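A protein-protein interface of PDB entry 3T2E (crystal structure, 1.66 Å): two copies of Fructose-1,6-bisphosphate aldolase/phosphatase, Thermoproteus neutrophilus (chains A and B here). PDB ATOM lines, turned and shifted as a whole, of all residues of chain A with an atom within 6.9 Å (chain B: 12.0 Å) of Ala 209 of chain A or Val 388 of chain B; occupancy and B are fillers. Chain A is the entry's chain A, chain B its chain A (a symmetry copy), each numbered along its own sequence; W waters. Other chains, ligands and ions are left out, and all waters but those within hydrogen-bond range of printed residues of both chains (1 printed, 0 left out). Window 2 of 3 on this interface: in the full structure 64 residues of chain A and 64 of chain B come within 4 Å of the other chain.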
ATOM      1  N   SER A 161      20.103   5.183 -19.792  1.00  0.00           N
ATOM      2  CA  SER A 161      19.020   4.789 -18.805  1.00  0.00           C
ATOM      3  C   SER A 161      18.953   5.562 -17.467  1.00  0.00           C
ATOM      4  O   SER A 161      17.962   5.487 -16.725  1.00  0.00           O
ATOM      5  CB  SER A 161      19.109   3.242 -18.559  1.00  0.00           C
ATOM      6  OG  SER A 161      20.193   2.947 -17.696  1.00  0.00           O
ATOM      7  N   GLU A 164      17.858  10.565 -16.633  1.00  0.00           N
ATOM      8  CA  GLU A 164      16.756  11.279 -16.041  1.00  0.00           C
ATOM      9  C   GLU A 164      16.985  11.633 -14.576  1.00  0.00           C
ATOM     10  O   GLU A 164      16.217  12.383 -13.998  1.00  0.00           O
ATOM     11  CB  GLU A 164      15.406  10.518 -16.160  1.00  0.00           C
ATOM     12  CG  GLU A 164      15.122   9.910 -17.651  1.00  0.00           C
ATOM     13  CD  GLU A 164      15.457  10.839 -18.837  1.00  0.00           C
ATOM     14  OE1 GLU A 164      15.172  12.076 -18.736  1.00  0.00           O
ATOM     15  OE2 GLU A 164      15.986  10.323 -19.880  1.00  0.00           O
ATOM     16  N   GLY A 165      17.998  11.038 -13.944  1.00  0.00           N
ATOM     17  CA  GLY A 165      18.343  11.445 -12.573  1.00  0.00           C
ATOM     18  C   GLY A 165      17.575  10.774 -11.471  1.00  0.00           C
ATOM     19  O   GLY A 165      16.977   9.678 -11.651  1.00  0.00           O
ATOM     20  N   PHE A 166      17.658  11.378 -10.301  1.00  0.00           N
ATOM     21  CA  PHE A 166      17.213  10.755  -9.055  1.00  0.00           C
ATOM     22  C   PHE A 166      16.466  11.684  -8.164  1.00  0.00           C
ATOM     23  O   PHE A 166      16.527  12.897  -8.345  1.00  0.00           O
ATOM     24  CB  PHE A 166      18.469  10.194  -8.266  1.00  0.00           C
ATOM     25  CG  PHE A 166      19.046   9.004  -8.974  1.00  0.00           C
ATOM     26  CD1 PHE A 166      18.556   7.727  -8.641  1.00  0.00           C
ATOM     27  CD2 PHE A 166      19.969   9.163 -10.027  1.00  0.00           C
ATOM     28  CE1 PHE A 166      19.016   6.584  -9.364  1.00  0.00           C
ATOM     29  CE2 PHE A 166      20.485   8.018 -10.707  1.00  0.00           C
ATOM     30  CZ  PHE A 166      19.969   6.774 -10.433  1.00  0.00           C
ATOM     31  N   ILE A 167      15.702  11.080  -7.241  1.00  0.00           N
ATOM     32  CA  ILE A 167      14.853  11.872  -6.298  1.00  0.00           C
ATOM     33  C   ILE A 167      15.418  11.605  -4.909  1.00  0.00           C
ATOM     34  O   ILE A 167      15.616  10.430  -4.490  1.00  0.00           O
ATOM     35  CB  ILE A 167      13.386  11.314  -6.267  1.00  0.00           C
ATOM     36  CG1 ILE A 167      12.797  11.436  -7.673  1.00  0.00           C
ATOM     37  CG2 ILE A 167      12.559  12.192  -5.270  1.00  0.00           C
ATOM     38  CD1 ILE A 167      11.474  10.525  -7.863  1.00  0.00           C
ATOM     39  N   LYS A 182      14.885  16.806  -6.865  1.00  0.00           N
ATOM     40  CA  LYS A 182      15.186  15.957  -8.071  1.00  0.00           C
ATOM     41  C   LYS A 182      16.441  16.477  -8.742  1.00  0.00           C
ATOM     42  O   LYS A 182      16.462  17.647  -9.148  1.00  0.00           O
ATOM     43  CB  LYS A 182      14.022  16.100  -9.087  1.00  0.00           C
ATOM     44  CG  LYS A 182      12.696  15.891  -8.397  1.00  0.00           C
ATOM     45  CD  LYS A 182      11.432  16.555  -9.135  1.00  0.00           C
ATOM     46  CE  LYS A 182      11.369  18.125  -9.382  1.00  0.00           C
ATOM     47  NZ  LYS A 182      11.468  19.058  -8.120  1.00  0.00           N
ATOM     48  N   PHE A 206      15.423   7.600  -4.711  1.00  0.00           N
ATOM     49  CA  PHE A 206      14.631   6.801  -5.676  1.00  0.00           C
ATOM     50  C   PHE A 206      15.049   7.156  -7.058  1.00  0.00           C
ATOM     51  O   PHE A 206      15.416   8.289  -7.368  1.00  0.00           O
ATOM     52  CB  PHE A 206      13.110   7.233  -5.487  1.00  0.00           C
ATOM     53  CG  PHE A 206      12.615   6.986  -4.135  1.00  0.00           C
ATOM     54  CD1 PHE A 206      12.124   5.697  -3.787  1.00  0.00           C
ATOM     55  CD2 PHE A 206      12.676   7.974  -3.148  1.00  0.00           C
ATOM     56  CE1 PHE A 206      11.703   5.394  -2.486  1.00  0.00           C
ATOM     57  CE2 PHE A 206      12.256   7.670  -1.840  1.00  0.00           C
ATOM     58  CZ  PHE A 206      11.758   6.399  -1.511  1.00  0.00           C
ATOM     59  N   ARG A 207      14.888   6.202  -7.989  1.00  0.00           N
ATOM     60  CA  ARG A 207      15.163   6.453  -9.377  1.00  0.00           C
ATOM     61  C   ARG A 207      14.017   7.314  -9.967  1.00  0.00           C
ATOM     62  O   ARG A 207      12.858   7.000  -9.697  1.00  0.00           O
ATOM     63  CB  ARG A 207      15.353   5.073 -10.076  1.00  0.00           C
ATOM     64  CG  ARG A 207      15.596   5.146 -11.533  1.00  0.00           C
ATOM     65  CD  ARG A 207      15.855   3.723 -12.030  1.00  0.00           C
ATOM     66  NE  ARG A 207      16.238   3.799 -13.412  1.00  0.00           N
ATOM     67  CZ  ARG A 207      16.119   2.813 -14.263  1.00  0.00           C
ATOM     68  NH1 ARG A 207      16.513   3.012 -15.510  1.00  0.00           N
ATOM     69  NH2 ARG A 207      15.586   1.645 -13.867  1.00  0.00           N
ATOM     70  N   ARG A 208      14.350   8.386 -10.708  1.00  0.00           N
ATOM     71  CA  ARG A 208      13.325   9.259 -11.359  1.00  0.00           C
ATOM     72  C   ARG A 208      12.540   8.531 -12.439  1.00  0.00           C
ATOM     73  O   ARG A 208      11.281   8.762 -12.597  1.00  0.00           O
ATOM     74  CB  ARG A 208      13.968  10.495 -11.941  1.00  0.00           C
ATOM     75  CG  ARG A 208      14.043  11.511 -10.873  1.00  0.00           C
ATOM     76  CD  ARG A 208      14.625  12.824 -11.375  1.00  0.00           C
ATOM     77  NE  ARG A 208      13.574  13.606 -12.061  1.00  0.00           N
ATOM     78  CZ  ARG A 208      13.818  14.804 -12.574  1.00  0.00           C
ATOM     79  NH1 ARG A 208      15.050  15.289 -12.454  1.00  0.00           N
ATOM     80  NH2 ARG A 208      12.877  15.515 -13.194  1.00  0.00           N
ATOM     81  N   ALA A 209      13.207   7.650 -13.148  1.00  0.00           N
ATOM     82  CA  ALA A 209      12.519   7.002 -14.356  1.00  0.00           C
ATOM     83  C   ALA A 209      11.217   6.287 -13.881  1.00  0.00           C
ATOM     84  O   ALA A 209      10.166   6.407 -14.580  1.00  0.00           O
ATOM     85  CB  ALA A 209      13.424   6.023 -15.142  1.00  0.00           C
ATOM     86  N   ASP A 210      11.256   5.568 -12.750  1.00  0.00           N
ATOM     87  CA  ASP A 210      10.211   4.627 -12.370  1.00  0.00           C
ATOM     88  C   ASP A 210       9.882   4.674 -10.889  1.00  0.00           C
ATOM     89  O   ASP A 210       9.002   3.958 -10.455  1.00  0.00           O
ATOM     90  CB  ASP A 210      10.549   3.210 -12.845  1.00  0.00           C
ATOM     91  CG  ASP A 210      11.783   2.634 -12.151  1.00  0.00           C
ATOM     92  OD1 ASP A 210      12.512   3.461 -11.478  1.00  0.00           O
ATOM     93  OD2 ASP A 210      12.095   1.423 -12.299  1.00  0.00           O
ATOM     94  N   GLY A 211      10.594   5.544 -10.097  1.00  0.00           N
ATOM     95  CA  GLY A 211      10.412   5.558  -8.678  1.00  0.00           C
ATOM     96  C   GLY A 211      11.032   4.413  -7.894  1.00  0.00           C
ATOM     97  O   GLY A 211      10.736   4.313  -6.678  1.00  0.00           O
ATOM     98  N   ALA A 212      11.891   3.620  -8.509  1.00  0.00           N
ATOM     99  CA  ALA A 212      12.485   2.401  -7.824  1.00  0.00           C
ATOM    100  C   ALA A 212      13.305   2.880  -6.603  1.00  0.00           C
ATOM    101  O   ALA A 212      14.026   3.834  -6.706  1.00  0.00           O
ATOM    102  CB  ALA A 212      13.359   1.573  -8.771  1.00  0.00           C
ATOM    103  N   TYR B 371       7.397  18.866   3.677  1.00  0.00           N
ATOM    104  CA  TYR B 371       6.300  18.064   4.124  1.00  0.00           C
ATOM    105  C   TYR B 371       6.522  17.827   5.568  1.00  0.00           C
ATOM    106  O   TYR B 371       7.598  17.396   5.959  1.00  0.00           O
ATOM    107  CB  TYR B 371       6.245  16.738   3.371  1.00  0.00           C
ATOM    108  CG  TYR B 371       6.077  16.886   1.889  1.00  0.00           C
ATOM    109  CD1 TYR B 371       4.799  16.920   1.309  1.00  0.00           C
ATOM    110  CD2 TYR B 371       7.183  16.957   1.019  1.00  0.00           C
ATOM    111  CE1 TYR B 371       4.637  17.058  -0.105  1.00  0.00           C
ATOM    112  CE2 TYR B 371       7.042  17.109  -0.355  1.00  0.00           C
ATOM    113  CZ  TYR B 371       5.760  17.143  -0.922  1.00  0.00           C
ATOM    114  OH  TYR B 371       5.633  17.276  -2.267  1.00  0.00           O
ATOM    115  N   TYR B 376       4.092  13.130   5.719  1.00  0.00           N
ATOM    116  CA  TYR B 376       4.871  12.575   4.581  1.00  0.00           C
ATOM    117  C   TYR B 376       5.004  11.045   4.643  1.00  0.00           C
ATOM    118  O   TYR B 376       4.845  10.356   3.628  1.00  0.00           O
ATOM    119  CB  TYR B 376       6.283  13.197   4.505  1.00  0.00           C
ATOM    120  CG  TYR B 376       7.129  12.527   3.433  1.00  0.00           C
ATOM    121  CD1 TYR B 376       7.091  13.027   2.161  1.00  0.00           C
ATOM    122  CD2 TYR B 376       7.953  11.398   3.713  1.00  0.00           C
ATOM    123  CE1 TYR B 376       7.813  12.444   1.119  1.00  0.00           C
ATOM    124  CE2 TYR B 376       8.704  10.809   2.670  1.00  0.00           C
ATOM    125  CZ  TYR B 376       8.648  11.353   1.422  1.00  0.00           C
ATOM    126  OH  TYR B 376       9.330  10.824   0.364  1.00  0.00           O
ATOM    127  N   ASP B 379       2.107   9.114   3.079  1.00  0.00           N
ATOM    128  CA  ASP B 379       1.873   9.351   1.665  1.00  0.00           C
ATOM    129  C   ASP B 379       3.157   9.322   0.811  1.00  0.00           C
ATOM    130  O   ASP B 379       3.141   9.836  -0.311  1.00  0.00           O
ATOM    131  CB  ASP B 379       1.237  10.713   1.461  1.00  0.00           C
ATOM    132  CG  ASP B 379      -0.097  10.896   2.254  1.00  0.00           C
ATOM    133  OD1 ASP B 379      -0.895   9.913   2.342  1.00  0.00           O
ATOM    134  OD2 ASP B 379      -0.288  12.032   2.794  1.00  0.00           O
ATOM    135  N   ARG B 380       4.252   8.757   1.349  1.00  0.00           N
ATOM    136  CA  ARG B 380       5.508   8.744   0.566  1.00  0.00           C
ATOM    137  C   ARG B 380       5.305   8.170  -0.855  1.00  0.00           C
ATOM    138  O   ARG B 380       5.687   8.786  -1.842  1.00  0.00           O
ATOM    139  CB  ARG B 380       6.567   7.925   1.275  1.00  0.00           C
ATOM    140  CG  ARG B 380       7.834   7.696   0.369  1.00  0.00           C
ATOM    141  CD  ARG B 380       8.810   6.754   1.051  1.00  0.00           C
ATOM    142  NE  ARG B 380       9.566   7.321   2.174  1.00  0.00           N
ATOM    143  CZ  ARG B 380       9.383   7.074   3.450  1.00  0.00           C
ATOM    144  NH1 ARG B 380       8.367   6.274   3.871  1.00  0.00           N
ATOM    145  NH2 ARG B 380      10.160   7.660   4.343  1.00  0.00           N
ATOM    146  N   LYS B 381       4.631   7.042  -0.936  1.00  0.00           N
ATOM    147  CA  LYS B 381       4.333   6.402  -2.204  1.00  0.00           C
ATOM    148  C   LYS B 381       3.640   7.334  -3.187  1.00  0.00           C
ATOM    149  O   LYS B 381       3.979   7.386  -4.324  1.00  0.00           O
ATOM    150  CB  LYS B 381       3.573   5.080  -1.991  1.00  0.00           C
ATOM    151  CG  LYS B 381       3.715   4.511  -0.531  1.00  0.00           C
ATOM    152  CD  LYS B 381       3.142   3.013  -0.225  1.00  0.00           C
ATOM    153  CE  LYS B 381       2.706   2.755   1.240  1.00  0.00           C
ATOM    154  NZ  LYS B 381       3.281   1.550   2.057  1.00  0.00           N
ATOM    155  N   LYS B 382       2.662   8.075  -2.707  1.00  0.00           N
ATOM    156  CA  LYS B 382       1.929   9.005  -3.527  1.00  0.00           C
ATOM    157  C   LYS B 382       2.801  10.173  -3.973  1.00  0.00           C
ATOM    158  O   LYS B 382       2.734  10.613  -5.161  1.00  0.00           O
ATOM    159  CB  LYS B 382       0.646   9.476  -2.735  1.00  0.00           C
ATOM    160  CG  LYS B 382      -0.121  10.684  -3.317  1.00  0.00           C
ATOM    161  CD  LYS B 382      -1.465  10.917  -2.526  1.00  0.00           C
ATOM    162  CE  LYS B 382      -1.392  12.020  -1.434  1.00  0.00           C
ATOM    163  NZ  LYS B 382      -1.193  13.369  -2.070  1.00  0.00           N
ATOM    164  N   TYR B 383       3.630  10.684  -3.041  1.00  0.00           N
ATOM    165  CA  TYR B 383       4.484  11.822  -3.402  1.00  0.00           C
ATOM    166  C   TYR B 383       5.523  11.433  -4.396  1.00  0.00           C
ATOM    167  O   TYR B 383       5.785  12.159  -5.357  1.00  0.00           O
ATOM    168  CB  TYR B 383       5.117  12.438  -2.166  1.00  0.00           C
ATOM    169  CG  TYR B 383       4.135  13.058  -1.210  1.00  0.00           C
ATOM    170  CD1 TYR B 383       3.153  13.983  -1.646  1.00  0.00           C
ATOM    171  CD2 TYR B 383       4.162  12.727   0.114  1.00  0.00           C
ATOM    172  CE1 TYR B 383       2.244  14.537  -0.733  1.00  0.00           C
ATOM    173  CE2 TYR B 383       3.250  13.269   1.045  1.00  0.00           C
ATOM    174  CZ  TYR B 383       2.302  14.163   0.614  1.00  0.00           C
ATOM    175  OH  TYR B 383       1.449  14.671   1.577  1.00  0.00           O
ATOM    176  N   ILE B 384       6.108  10.234  -4.217  1.00  0.00           N
ATOM    177  CA  ILE B 384       7.089   9.764  -5.231  1.00  0.00           C
ATOM    178  C   ILE B 384       6.447   9.547  -6.590  1.00  0.00           C
ATOM    179  O   ILE B 384       7.013   9.952  -7.623  1.00  0.00           O
ATOM    180  CB  ILE B 384       7.873   8.493  -4.801  1.00  0.00           C
ATOM    181  CG1 ILE B 384       8.580   8.703  -3.450  1.00  0.00           C
ATOM    182  CG2 ILE B 384       8.756   8.024  -5.914  1.00  0.00           C
ATOM    183  CD1 ILE B 384       9.540   9.878  -3.377  1.00  0.00           C
ATOM    184  N   GLU B 385       5.278   8.891  -6.641  1.00  0.00           N
ATOM    185  CA  GLU B 385       4.612   8.733  -7.965  1.00  0.00           C
ATOM    186  C   GLU B 385       4.310  10.050  -8.652  1.00  0.00           C
ATOM    187  O   GLU B 385       4.517  10.146  -9.844  1.00  0.00           O
ATOM    188  CB  GLU B 385       3.343   7.904  -7.858  1.00  0.00           C
ATOM    189  CG  GLU B 385       3.652   6.473  -7.472  1.00  0.00           C
ATOM    190  CD  GLU B 385       2.409   5.621  -7.269  1.00  0.00           C
ATOM    191  OE1 GLU B 385       1.264   6.164  -7.385  1.00  0.00           O
ATOM    192  OE2 GLU B 385       2.596   4.406  -6.997  1.00  0.00           O
ATOM    193  N   ALA B 386       3.899  11.056  -7.884  1.00  0.00           N
ATOM    194  CA  ALA B 386       3.715  12.422  -8.387  1.00  0.00           C
ATOM    195  C   ALA B 386       4.955  12.940  -9.068  1.00  0.00           C
ATOM    196  O   ALA B 386       4.897  13.371 -10.214  1.00  0.00           O
ATOM    197  CB  ALA B 386       3.258  13.355  -7.289  1.00  0.00           C
ATOM    198  N   VAL B 387       6.111  12.847  -8.391  1.00  0.00           N
ATOM    199  CA  VAL B 387       7.372  13.305  -9.029  1.00  0.00           C
ATOM    200  C   VAL B 387       7.720  12.493 -10.277  1.00  0.00           C
ATOM    201  O   VAL B 387       8.172  13.050 -11.322  1.00  0.00           O
ATOM    202  CB  VAL B 387       8.598  13.224  -8.007  1.00  0.00           C
ATOM    203  CG1 VAL B 387       9.909  13.604  -8.704  1.00  0.00           C
ATOM    204  CG2 VAL B 387       8.375  14.044  -6.754  1.00  0.00           C
ATOM    205  N   VAL B 388       7.519  11.170 -10.224  1.00  0.00           N
ATOM    206  CA  VAL B 388       7.857  10.321 -11.352  1.00  0.00           C
ATOM    207  C   VAL B 388       6.978  10.652 -12.582  1.00  0.00           C
ATOM    208  O   VAL B 388       7.491  10.820 -13.707  1.00  0.00           O
ATOM    209  CB  VAL B 388       7.773   8.823 -10.968  1.00  0.00           C
ATOM    210  CG1 VAL B 388       7.927   7.873 -12.189  1.00  0.00           C
ATOM    211  CG2 VAL B 388       8.830   8.488  -9.868  1.00  0.00           C
ATOM    212  N   LYS B 389       5.662  10.751 -12.345  1.00  0.00           N
ATOM    213  CA  LYS B 389       4.667  11.180 -13.362  1.00  0.00           C
ATOM    214  C   LYS B 389       4.909  12.622 -13.852  1.00  0.00           C
ATOM    215  O   LYS B 389       5.237  12.833 -15.031  1.00  0.00           O
ATOM    216  CB  LYS B 389       3.255  11.046 -12.798  1.00  0.00           C
ATOM    217  CG  LYS B 389       2.515   9.752 -13.215  1.00  0.00           C
ATOM    218  CD  LYS B 389       2.469   8.643 -12.126  1.00  0.00           C
ATOM    219  CE  LYS B 389       1.020   8.173 -11.920  1.00  0.00           C
ATOM    220  NZ  LYS B 389       0.936   6.753 -11.524  1.00  0.00           N
HETATM  221  O   HOH W   1      10.169  10.360 -14.371  1.00  0.00           O
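No residue of chain B comes within 4 Å of Glu 164 of chain A.
No residue of chain B comes within 4 Å of Phe 166 of chain A.
Of the printed residues of chain B, Arg 208 of chain A touches Val 388.
Ala 209 of chain A touches just one residue of chain B: Val 388 (3.6 Å).
Asp 210 of chain A touches just one residue of chain B: Val 388.
Gly 211 of chain A touches just one residue of chain B: Val 388 (3.4 Å).
Printed residues of chain A within 4 Å of Val 387 of chain B: Ile 167 (3.6 Å) and Lys 182 (3.3 Å).
Of the printed residues of chain A, Val 388 of chain B touches Ile 167, Arg 208, Ala 209, Asp 210 and Gly 211.
The nearest residue of chain B that does not touch Ala 209 of chain A is Lys 389 of chain B (6.6 Å).
Of the 13 printed residues of chain A, 7 touch a printed residue of chain B.
Of the 13 printed residues of chain B, 4 touch a printed residue of chain A.
Printed residues of chain B that touch a printed residue of chain A: Arg 380, Ile 384, Val 387 and Val 388.
Hydrophobic or aromatic side chains of chain B that line the printed part of chain A: Ile 384, Val 387 and Val 388.
Among the printed residues, 9 pairs touch across the chains.
Among the printed residues, no Asp or Glu carboxylate lies within 4 Å of a Lys or Arg side-chain nitrogen of the other chain.
Water W1 lies within hydrogen-bond range of the backbone carbonyl oxygen of Arg 208 of chain A and the backbone carbonyl oxygen of Val 388 of chain B.
CD1 of Ile 167 of chain A touches CG1 of Val 387 of chain B, at 3.6 Å.
Ile 167 of chain A touches Val 388 of chain B.
Val 387 of chain B touches Lys 182 of chain A (CG1 to CD, 3.3 Å).
Phe 206 of chain A touches Arg 380 of chain B (CZ to CD, 3.9 Å).
Phe 206 of chain A touches Ile 384 of chain B.
Arg 208 of chain A touches Val 388 of chain B (O to CG1, 3.5 Å).
Val 388 of chain B touches Ala 209 of chain A (CG1 to O, 3.6 Å).
Asp 210 of chain A touches Val 388 of chain B.
N of Gly 211 of chain A touches CG2 of Val 388 of chain B, 3.4 Å away.
No position is printed for both chains.
Of the 9 pairs that touch across the chains among the printed residues, none has its exchanged pair printed and touching as well.
O of Phe 206 of chain A lies within hydrogen-bond range of N of Ile 167 of chain A (2.8 Å).
OD1 of Asp 210 of chain A is in hydrogen-bond range of N of Ala 212 of chain A (3.0 Å).
The backbone carbonyl oxygen of Glu 164 of chain A lies close to the guanidinium group of Arg 208 of chain A.
OD2 of Asp 210 of chain A lies within salt-bridge range of NH2 of Arg 207 of chain A, at 3.8 Å.
The backbone NH (N) of Arg 208 of chain A is in hydrogen-bond range of the backbone carbonyl oxygen (O) of Gly 165 of chain A, 3.1 Å away.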
